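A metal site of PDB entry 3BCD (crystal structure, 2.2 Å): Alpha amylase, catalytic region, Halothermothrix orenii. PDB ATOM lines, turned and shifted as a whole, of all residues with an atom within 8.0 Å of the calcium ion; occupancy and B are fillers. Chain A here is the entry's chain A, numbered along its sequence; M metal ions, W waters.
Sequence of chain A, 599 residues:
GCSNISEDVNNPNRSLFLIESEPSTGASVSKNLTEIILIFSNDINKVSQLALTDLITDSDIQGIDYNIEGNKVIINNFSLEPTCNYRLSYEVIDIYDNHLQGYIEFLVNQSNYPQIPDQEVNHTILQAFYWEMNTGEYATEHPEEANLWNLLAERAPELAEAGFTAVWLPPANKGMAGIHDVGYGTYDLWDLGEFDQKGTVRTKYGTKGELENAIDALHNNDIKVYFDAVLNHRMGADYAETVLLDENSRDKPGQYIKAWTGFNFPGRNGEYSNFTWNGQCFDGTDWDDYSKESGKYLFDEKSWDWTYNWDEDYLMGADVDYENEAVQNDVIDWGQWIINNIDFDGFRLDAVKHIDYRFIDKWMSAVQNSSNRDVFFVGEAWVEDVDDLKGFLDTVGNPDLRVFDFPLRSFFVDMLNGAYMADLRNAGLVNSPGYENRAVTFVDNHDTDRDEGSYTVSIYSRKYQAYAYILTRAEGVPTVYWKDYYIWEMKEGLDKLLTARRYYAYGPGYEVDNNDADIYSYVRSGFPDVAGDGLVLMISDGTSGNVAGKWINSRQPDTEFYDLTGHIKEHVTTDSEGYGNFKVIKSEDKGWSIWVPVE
The calcium ion is bound by OD1 of Asp 319, 2.3 Å away. O of Asp 313 binds the calcium ion (2.3 Å). The calcium ion is bound by OD1 of Asn 232 (2.3 Å). OD1 of Asp 313 binds the calcium ion (2.3 Å). The calcium ion is bound by O of His 354 (2.3 Å). The calcium ion is bound by water W1. The calcium ion has six donor atoms within binding distance.
Within 4 Å of the calcium ion: Asn 232, Asp 313, Asp 319 and His 354.
The backbone carbonyl oxygen of Asp 319 lies within hydrogen-bond range of the backbone NH of Asp 283 (3.1 Å). ND2 of Asn 232 lies within hydrogen-bond range of ND1 of His 233 (2.9 Å). N of Val 320 is in hydrogen-bond range of O of Asn 232 (3.1 Å). The backbone carbonyl oxygen of Glu 312 sits at hydrogen-bond distance from a ring nitrogen (ND1) of His 354, 2.7 Å away. The side-chain carboxylate of Asp 313 lies within hydrogen-bond range of the backbone NH of Asp 305.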
ATOM      1  N   LEU A 231      -6.457  13.090 -15.307  1.00  0.00           N
ATOM      2  CA  LEU A 231      -5.113  13.467 -15.847  1.00  0.00           C
ATOM      3  C   LEU A 231      -4.739  15.003 -15.822  1.00  0.00           C
ATOM      4  O   LEU A 231      -3.610  15.358 -16.144  1.00  0.00           O
ATOM      5  CB  LEU A 231      -4.946  12.897 -17.280  1.00  0.00           C
ATOM      6  CG  LEU A 231      -5.170  11.422 -17.594  1.00  0.00           C
ATOM      7  CD1 LEU A 231      -5.082  11.162 -19.121  1.00  0.00           C
ATOM      8  CD2 LEU A 231      -4.212  10.521 -16.811  1.00  0.00           C
ATOM      9  N   ASN A 232      -5.655  15.881 -15.386  1.00  0.00           N
ATOM     10  CA  ASN A 232      -5.522  17.355 -15.528  1.00  0.00           C
ATOM     11  C   ASN A 232      -4.505  17.925 -14.543  1.00  0.00           C
ATOM     12  O   ASN A 232      -3.678  18.746 -14.932  1.00  0.00           O
ATOM     13  CB  ASN A 232      -6.884  18.097 -15.248  1.00  0.00           C
ATOM     14  CG  ASN A 232      -6.693  19.586 -15.105  1.00  0.00           C
ATOM     15  OD1 ASN A 232      -6.278  20.241 -16.057  1.00  0.00           O
ATOM     16  ND2 ASN A 232      -6.866  20.138 -13.840  1.00  0.00           N
ATOM     17  N   HIS A 233      -4.590  17.533 -13.267  1.00  0.00           N
ATOM     18  CA  HIS A 233      -3.819  18.149 -12.210  1.00  0.00           C
ATOM     19  C   HIS A 233      -3.267  17.096 -11.235  1.00  0.00           C
ATOM     20  O   HIS A 233      -3.551  15.903 -11.363  1.00  0.00           O
ATOM     21  CB  HIS A 233      -4.721  19.065 -11.427  1.00  0.00           C
ATOM     22  CG  HIS A 233      -5.927  18.364 -10.917  1.00  0.00           C
ATOM     23  ND1 HIS A 233      -7.143  18.357 -11.593  1.00  0.00           N
ATOM     24  CD2 HIS A 233      -6.087  17.525  -9.860  1.00  0.00           C
ATOM     25  CE1 HIS A 233      -8.003  17.594 -10.928  1.00  0.00           C
ATOM     26  NE2 HIS A 233      -7.381  17.077  -9.874  1.00  0.00           N
ATOM     27  N   ASP A 283       2.690  23.622 -15.467  1.00  0.00           N
ATOM     28  CA  ASP A 283       2.596  24.940 -16.070  1.00  0.00           C
ATOM     29  C   ASP A 283       2.255  25.955 -14.956  1.00  0.00           C
ATOM     30  O   ASP A 283       2.625  27.116 -14.999  1.00  0.00           O
ATOM     31  CB  ASP A 283       1.454  24.951 -17.106  1.00  0.00           C
ATOM     32  CG  ASP A 283       1.839  24.331 -18.480  1.00  0.00           C
ATOM     33  OD1 ASP A 283       2.998  24.415 -18.905  1.00  0.00           O
ATOM     34  OD2 ASP A 283       0.962  23.762 -19.178  1.00  0.00           O
ATOM     35  N   TRP A 304       0.471  27.702 -21.136  1.00  0.00           N
ATOM     36  CA  TRP A 304      -0.689  26.880 -21.051  1.00  0.00           C
ATOM     37  C   TRP A 304      -0.802  26.079 -22.328  1.00  0.00           C
ATOM     38  O   TRP A 304      -0.445  26.561 -23.412  1.00  0.00           O
ATOM     39  CB  TRP A 304      -1.924  27.744 -20.864  1.00  0.00           C
ATOM     40  CG  TRP A 304      -1.939  28.583 -19.615  1.00  0.00           C
ATOM     41  CD1 TRP A 304      -2.142  29.909 -19.579  1.00  0.00           C
ATOM     42  CD2 TRP A 304      -1.837  28.162 -18.254  1.00  0.00           C
ATOM     43  NE1 TRP A 304      -2.144  30.368 -18.292  1.00  0.00           N
ATOM     44  CE2 TRP A 304      -1.931  29.311 -17.452  1.00  0.00           C
ATOM     45  CE3 TRP A 304      -1.645  26.903 -17.626  1.00  0.00           C
ATOM     46  CZ2 TRP A 304      -1.857  29.265 -16.025  1.00  0.00           C
ATOM     47  CZ3 TRP A 304      -1.534  26.856 -16.254  1.00  0.00           C
ATOM     48  CH2 TRP A 304      -1.663  28.033 -15.440  1.00  0.00           C
ATOM     49  N   ASP A 305      -1.337  24.863 -22.215  1.00  0.00           N
ATOM     50  CA  ASP A 305      -1.393  23.926 -23.330  1.00  0.00           C
ATOM     51  C   ASP A 305      -2.527  24.237 -24.207  1.00  0.00           C
ATOM     52  O   ASP A 305      -3.434  24.978 -23.826  1.00  0.00           O
ATOM     53  CB  ASP A 305      -1.421  22.495 -22.816  1.00  0.00           C
ATOM     54  CG  ASP A 305      -0.260  22.208 -21.811  1.00  0.00           C
ATOM     55  OD1 ASP A 305       0.826  22.726 -22.099  1.00  0.00           O
ATOM     56  OD2 ASP A 305      -0.417  21.492 -20.764  1.00  0.00           O
ATOM     57  N   THR A 307      -5.883  24.181 -25.796  1.00  0.00           N
ATOM     58  CA  THR A 307      -7.185  23.615 -25.513  1.00  0.00           C
ATOM     59  C   THR A 307      -8.178  24.126 -26.470  1.00  0.00           C
ATOM     60  O   THR A 307      -7.990  25.145 -27.080  1.00  0.00           O
ATOM     61  CB  THR A 307      -7.624  23.994 -24.105  1.00  0.00           C
ATOM     62  OG1 THR A 307      -7.478  25.382 -23.924  1.00  0.00           O
ATOM     63  CG2 THR A 307      -6.756  23.341 -23.081  1.00  0.00           C
ATOM     64  N   GLU A 312      -8.428  27.653 -21.101  1.00  0.00           N
ATOM     65  CA  GLU A 312      -9.128  26.675 -20.278  1.00  0.00           C
ATOM     66  C   GLU A 312      -8.202  25.588 -19.840  1.00  0.00           C
ATOM     67  O   GLU A 312      -8.664  24.600 -19.409  1.00  0.00           O
ATOM     68  CB  GLU A 312     -10.304  26.029 -21.044  1.00  0.00           C
ATOM     69  CG  GLU A 312     -11.629  26.671 -20.652  1.00  0.00           C
ATOM     70  CD  GLU A 312     -12.824  26.197 -21.416  1.00  0.00           C
ATOM     71  OE1 GLU A 312     -12.776  25.154 -22.130  1.00  0.00           O
ATOM     72  OE2 GLU A 312     -13.823  26.906 -21.282  1.00  0.00           O
ATOM     73  N   ASP A 313      -6.892  25.764 -19.903  1.00  0.00           N
ATOM     74  CA  ASP A 313      -6.013  24.717 -19.386  1.00  0.00           C
ATOM     75  C   ASP A 313      -6.071  24.790 -17.848  1.00  0.00           C
ATOM     76  O   ASP A 313      -6.114  23.751 -17.189  1.00  0.00           O
ATOM     77  CB  ASP A 313      -4.593  24.876 -19.963  1.00  0.00           C
ATOM     78  CG  ASP A 313      -3.618  23.724 -19.584  1.00  0.00           C
ATOM     79  OD1 ASP A 313      -3.969  22.564 -19.238  1.00  0.00           O
ATOM     80  OD2 ASP A 313      -2.428  24.000 -19.677  1.00  0.00           O
ATOM     81  N   TYR A 314      -6.027  25.970 -17.244  1.00  0.00           N
ATOM     82  CA  TYR A 314      -6.032  25.999 -15.762  1.00  0.00           C
ATOM     83  C   TYR A 314      -7.445  25.744 -15.187  1.00  0.00           C
ATOM     84  O   TYR A 314      -8.384  26.448 -15.567  1.00  0.00           O
ATOM     85  CB  TYR A 314      -5.476  27.296 -15.138  1.00  0.00           C
ATOM     86  CG  TYR A 314      -5.245  26.997 -13.661  1.00  0.00           C
ATOM     87  CD1 TYR A 314      -4.166  26.160 -13.280  1.00  0.00           C
ATOM     88  CD2 TYR A 314      -6.118  27.429 -12.654  1.00  0.00           C
ATOM     89  CE1 TYR A 314      -3.970  25.780 -11.974  1.00  0.00           C
ATOM     90  CE2 TYR A 314      -5.904  27.056 -11.324  1.00  0.00           C
ATOM     91  CZ  TYR A 314      -4.813  26.226 -11.015  1.00  0.00           C
ATOM     92  OH  TYR A 314      -4.575  25.804  -9.730  1.00  0.00           O
ATOM     93  N   LEU A 315      -7.579  24.746 -14.304  1.00  0.00           N
ATOM     94  CA  LEU A 315      -8.826  24.480 -13.534  1.00  0.00           C
ATOM     95  C   LEU A 315      -8.562  24.541 -11.994  1.00  0.00           C
ATOM     96  O   LEU A 315      -9.152  25.317 -11.305  1.00  0.00           O
ATOM     97  CB  LEU A 315      -9.438  23.133 -13.915  1.00  0.00           C
ATOM     98  CG  LEU A 315     -10.806  22.709 -13.362  1.00  0.00           C
ATOM     99  CD1 LEU A 315     -11.991  23.700 -13.708  1.00  0.00           C
ATOM    100  CD2 LEU A 315     -11.168  21.291 -13.828  1.00  0.00           C
ATOM    101  N   MET A 316      -7.699  23.678 -11.470  1.00  0.00           N
ATOM    102  CA  MET A 316      -7.412  23.633  -9.989  1.00  0.00           C
ATOM    103  C   MET A 316      -6.139  22.875  -9.816  1.00  0.00           C
ATOM    104  O   MET A 316      -5.704  22.209 -10.749  1.00  0.00           O
ATOM    105  CB  MET A 316      -8.499  22.874  -9.275  1.00  0.00           C
ATOM    106  CG  MET A 316      -8.873  21.547 -10.024  1.00  0.00           C
ATOM    107  SD  MET A 316     -10.051  20.426  -9.201  1.00  0.00           S
ATOM    108  CE  MET A 316     -11.615  21.276  -9.534  1.00  0.00           C
ATOM    109  N   ALA A 318      -2.056  21.672  -8.948  1.00  0.00           N
ATOM    110  CA  ALA A 318      -0.861  21.943  -9.681  1.00  0.00           C
ATOM    111  C   ALA A 318      -1.209  21.476 -11.142  1.00  0.00           C
ATOM    112  O   ALA A 318      -1.493  20.287 -11.349  1.00  0.00           O
ATOM    113  CB  ALA A 318       0.293  21.186  -9.097  1.00  0.00           C
ATOM    114  N   ASP A 319      -1.166  22.341 -12.139  1.00  0.00           N
ATOM    115  CA  ASP A 319      -1.687  21.975 -13.515  1.00  0.00           C
ATOM    116  C   ASP A 319      -0.592  21.275 -14.268  1.00  0.00           C
ATOM    117  O   ASP A 319       0.491  21.755 -14.276  1.00  0.00           O
ATOM    118  CB  ASP A 319      -2.059  23.196 -14.328  1.00  0.00           C
ATOM    119  CG  ASP A 319      -2.677  22.847 -15.725  1.00  0.00           C
ATOM    120  OD1 ASP A 319      -3.907  22.533 -15.683  1.00  0.00           O
ATOM    121  OD2 ASP A 319      -1.975  22.972 -16.826  1.00  0.00           O
ATOM    122  N   VAL A 320      -0.871  20.160 -14.921  1.00  0.00           N
ATOM    123  CA  VAL A 320       0.194  19.370 -15.544  1.00  0.00           C
ATOM    124  C   VAL A 320       0.639  19.997 -16.838  1.00  0.00           C
ATOM    125  O   VAL A 320      -0.181  20.507 -17.574  1.00  0.00           O
ATOM    126  CB  VAL A 320      -0.252  17.910 -15.838  1.00  0.00           C
ATOM    127  CG1 VAL A 320       0.838  17.103 -16.595  1.00  0.00           C
ATOM    128  CG2 VAL A 320      -0.650  17.200 -14.563  1.00  0.00           C
ATOM    129  N   ASP A 321       1.939  19.931 -17.134  1.00  0.00           N
ATOM    130  CA  ASP A 321       2.448  20.461 -18.371  1.00  0.00           C
ATOM    131  C   ASP A 321       2.577  19.345 -19.372  1.00  0.00           C
ATOM    132  O   ASP A 321       3.566  18.625 -19.300  1.00  0.00           O
ATOM    133  CB  ASP A 321       3.799  21.170 -18.156  1.00  0.00           C
ATOM    134  CG  ASP A 321       4.421  21.724 -19.491  1.00  0.00           C
ATOM    135  OD1 ASP A 321       3.707  21.816 -20.524  1.00  0.00           O
ATOM    136  OD2 ASP A 321       5.630  22.032 -19.491  1.00  0.00           O
ATOM    137  N   TYR A 322       1.613  19.201 -20.289  1.00  0.00           N
ATOM    138  CA  TYR A 322       1.687  18.148 -21.328  1.00  0.00           C
ATOM    139  C   TYR A 322       2.556  18.485 -22.533  1.00  0.00           C
ATOM    140  O   TYR A 322       2.635  17.686 -23.484  1.00  0.00           O
ATOM    141  CB  TYR A 322       0.280  17.637 -21.736  1.00  0.00           C
ATOM    142  CG  TYR A 322      -0.249  16.742 -20.665  1.00  0.00           C
ATOM    143  CD1 TYR A 322      -1.305  17.132 -19.851  1.00  0.00           C
ATOM    144  CD2 TYR A 322       0.408  15.543 -20.358  1.00  0.00           C
ATOM    145  CE1 TYR A 322      -1.737  16.301 -18.800  1.00  0.00           C
ATOM    146  CE2 TYR A 322       0.008  14.730 -19.311  1.00  0.00           C
ATOM    147  CZ  TYR A 322      -1.056  15.111 -18.525  1.00  0.00           C
ATOM    148  OH  TYR A 322      -1.471  14.283 -17.491  1.00  0.00           O
ATOM    149  N   ALA A 351     -12.550  15.895 -17.092  1.00  0.00           N
ATOM    150  CA  ALA A 351     -12.181  17.301 -17.374  1.00  0.00           C
ATOM    151  C   ALA A 351     -11.460  17.397 -18.703  1.00  0.00           C
ATOM    152  O   ALA A 351     -10.432  18.084 -18.821  1.00  0.00           O
ATOM    153  CB  ALA A 351     -11.276  17.871 -16.221  1.00  0.00           C
ATOM    154  N   VAL A 352     -11.939  16.664 -19.701  1.00  0.00           N
ATOM    155  CA  VAL A 352     -11.121  16.406 -20.884  1.00  0.00           C
ATOM    156  C   VAL A 352     -10.891  17.730 -21.645  1.00  0.00           C
ATOM    157  O   VAL A 352      -9.908  17.874 -22.367  1.00  0.00           O
ATOM    158  CB  VAL A 352     -11.733  15.296 -21.732  1.00  0.00           C
ATOM    159  CG1 VAL A 352     -13.002  15.800 -22.468  1.00  0.00           C
ATOM    160  CG2 VAL A 352     -10.727  14.681 -22.585  1.00  0.00           C
ATOM    161  N   LYS A 353     -11.691  18.740 -21.423  1.00  0.00           N
ATOM    162  CA  LYS A 353     -11.504  19.951 -22.209  1.00  0.00           C
ATOM    163  C   LYS A 353     -10.434  20.885 -21.631  1.00  0.00           C
ATOM    164  O   LYS A 353      -9.965  21.813 -22.319  1.00  0.00           O
ATOM    165  CB  LYS A 353     -12.871  20.647 -22.507  1.00  0.00           C
ATOM    166  CG  LYS A 353     -13.418  21.430 -21.348  1.00  0.00           C
ATOM    167  CD  LYS A 353     -14.820  22.133 -21.626  1.00  0.00           C
ATOM    168  CE  LYS A 353     -15.244  22.907 -20.393  1.00  0.00           C
ATOM    169  NZ  LYS A 353     -16.482  23.701 -20.610  1.00  0.00           N
ATOM    170  N   HIS A 354      -9.989  20.622 -20.389  1.00  0.00           N
ATOM    171  CA  HIS A 354      -8.857  21.366 -19.798  1.00  0.00           C
ATOM    172  C   HIS A 354      -7.503  20.732 -19.926  1.00  0.00           C
ATOM    173  O   HIS A 354      -6.589  21.037 -19.159  1.00  0.00           O
ATOM    174  CB  HIS A 354      -9.112  21.611 -18.302  1.00  0.00           C
ATOM    175  CG  HIS A 354     -10.472  22.130 -18.022  1.00  0.00           C
ATOM    176  ND1 HIS A 354     -10.799  23.460 -18.136  1.00  0.00           N
ATOM    177  CD2 HIS A 354     -11.601  21.500 -17.605  1.00  0.00           C
ATOM    178  CE1 HIS A 354     -12.072  23.635 -17.831  1.00  0.00           C
ATOM    179  NE2 HIS A 354     -12.590  22.459 -17.516  1.00  0.00           N
ATOM    180  N   ILE A 355      -7.383  19.844 -20.914  1.00  0.00           N
ATOM    181  CA  ILE A 355      -6.138  19.051 -21.141  1.00  0.00           C
ATOM    182  C   ILE A 355      -5.747  19.189 -22.591  1.00  0.00           C
ATOM    183  O   ILE A 355      -6.573  19.116 -23.532  1.00  0.00           O
ATOM    184  CB  ILE A 355      -6.245  17.511 -20.674  1.00  0.00           C
ATOM    185  CG1 ILE A 355      -6.529  17.440 -19.171  1.00  0.00           C
ATOM    186  CG2 ILE A 355      -4.945  16.657 -20.974  1.00  0.00           C
ATOM    187  CD1 ILE A 355      -7.047  16.107 -18.702  1.00  0.00           C
ATOM    188  N   ASP A 356      -4.477  19.520 -22.761  1.00  0.00           N
ATOM    189  CA  ASP A 356      -3.890  19.633 -24.054  1.00  0.00           C
ATOM    190  C   ASP A 356      -4.523  18.656 -25.041  1.00  0.00           C
ATOM    191  O   ASP A 356      -4.332  17.488 -24.929  1.00  0.00           O
ATOM    192  CB  ASP A 356      -2.412  19.344 -23.888  1.00  0.00           C
ATOM    193  CG  ASP A 356      -1.596  19.727 -25.115  1.00  0.00           C
ATOM    194  OD1 ASP A 356      -1.921  19.288 -26.230  1.00  0.00           O
ATOM    195  OD2 ASP A 356      -0.563  20.420 -24.949  1.00  0.00           O
HETATM  196 CA    CA M   1      -5.127  21.682 -17.445  1.00  0.00          CA
HETATM  197  O   HOH W   1      -3.690  19.761 -17.806  1.00  0.00           O
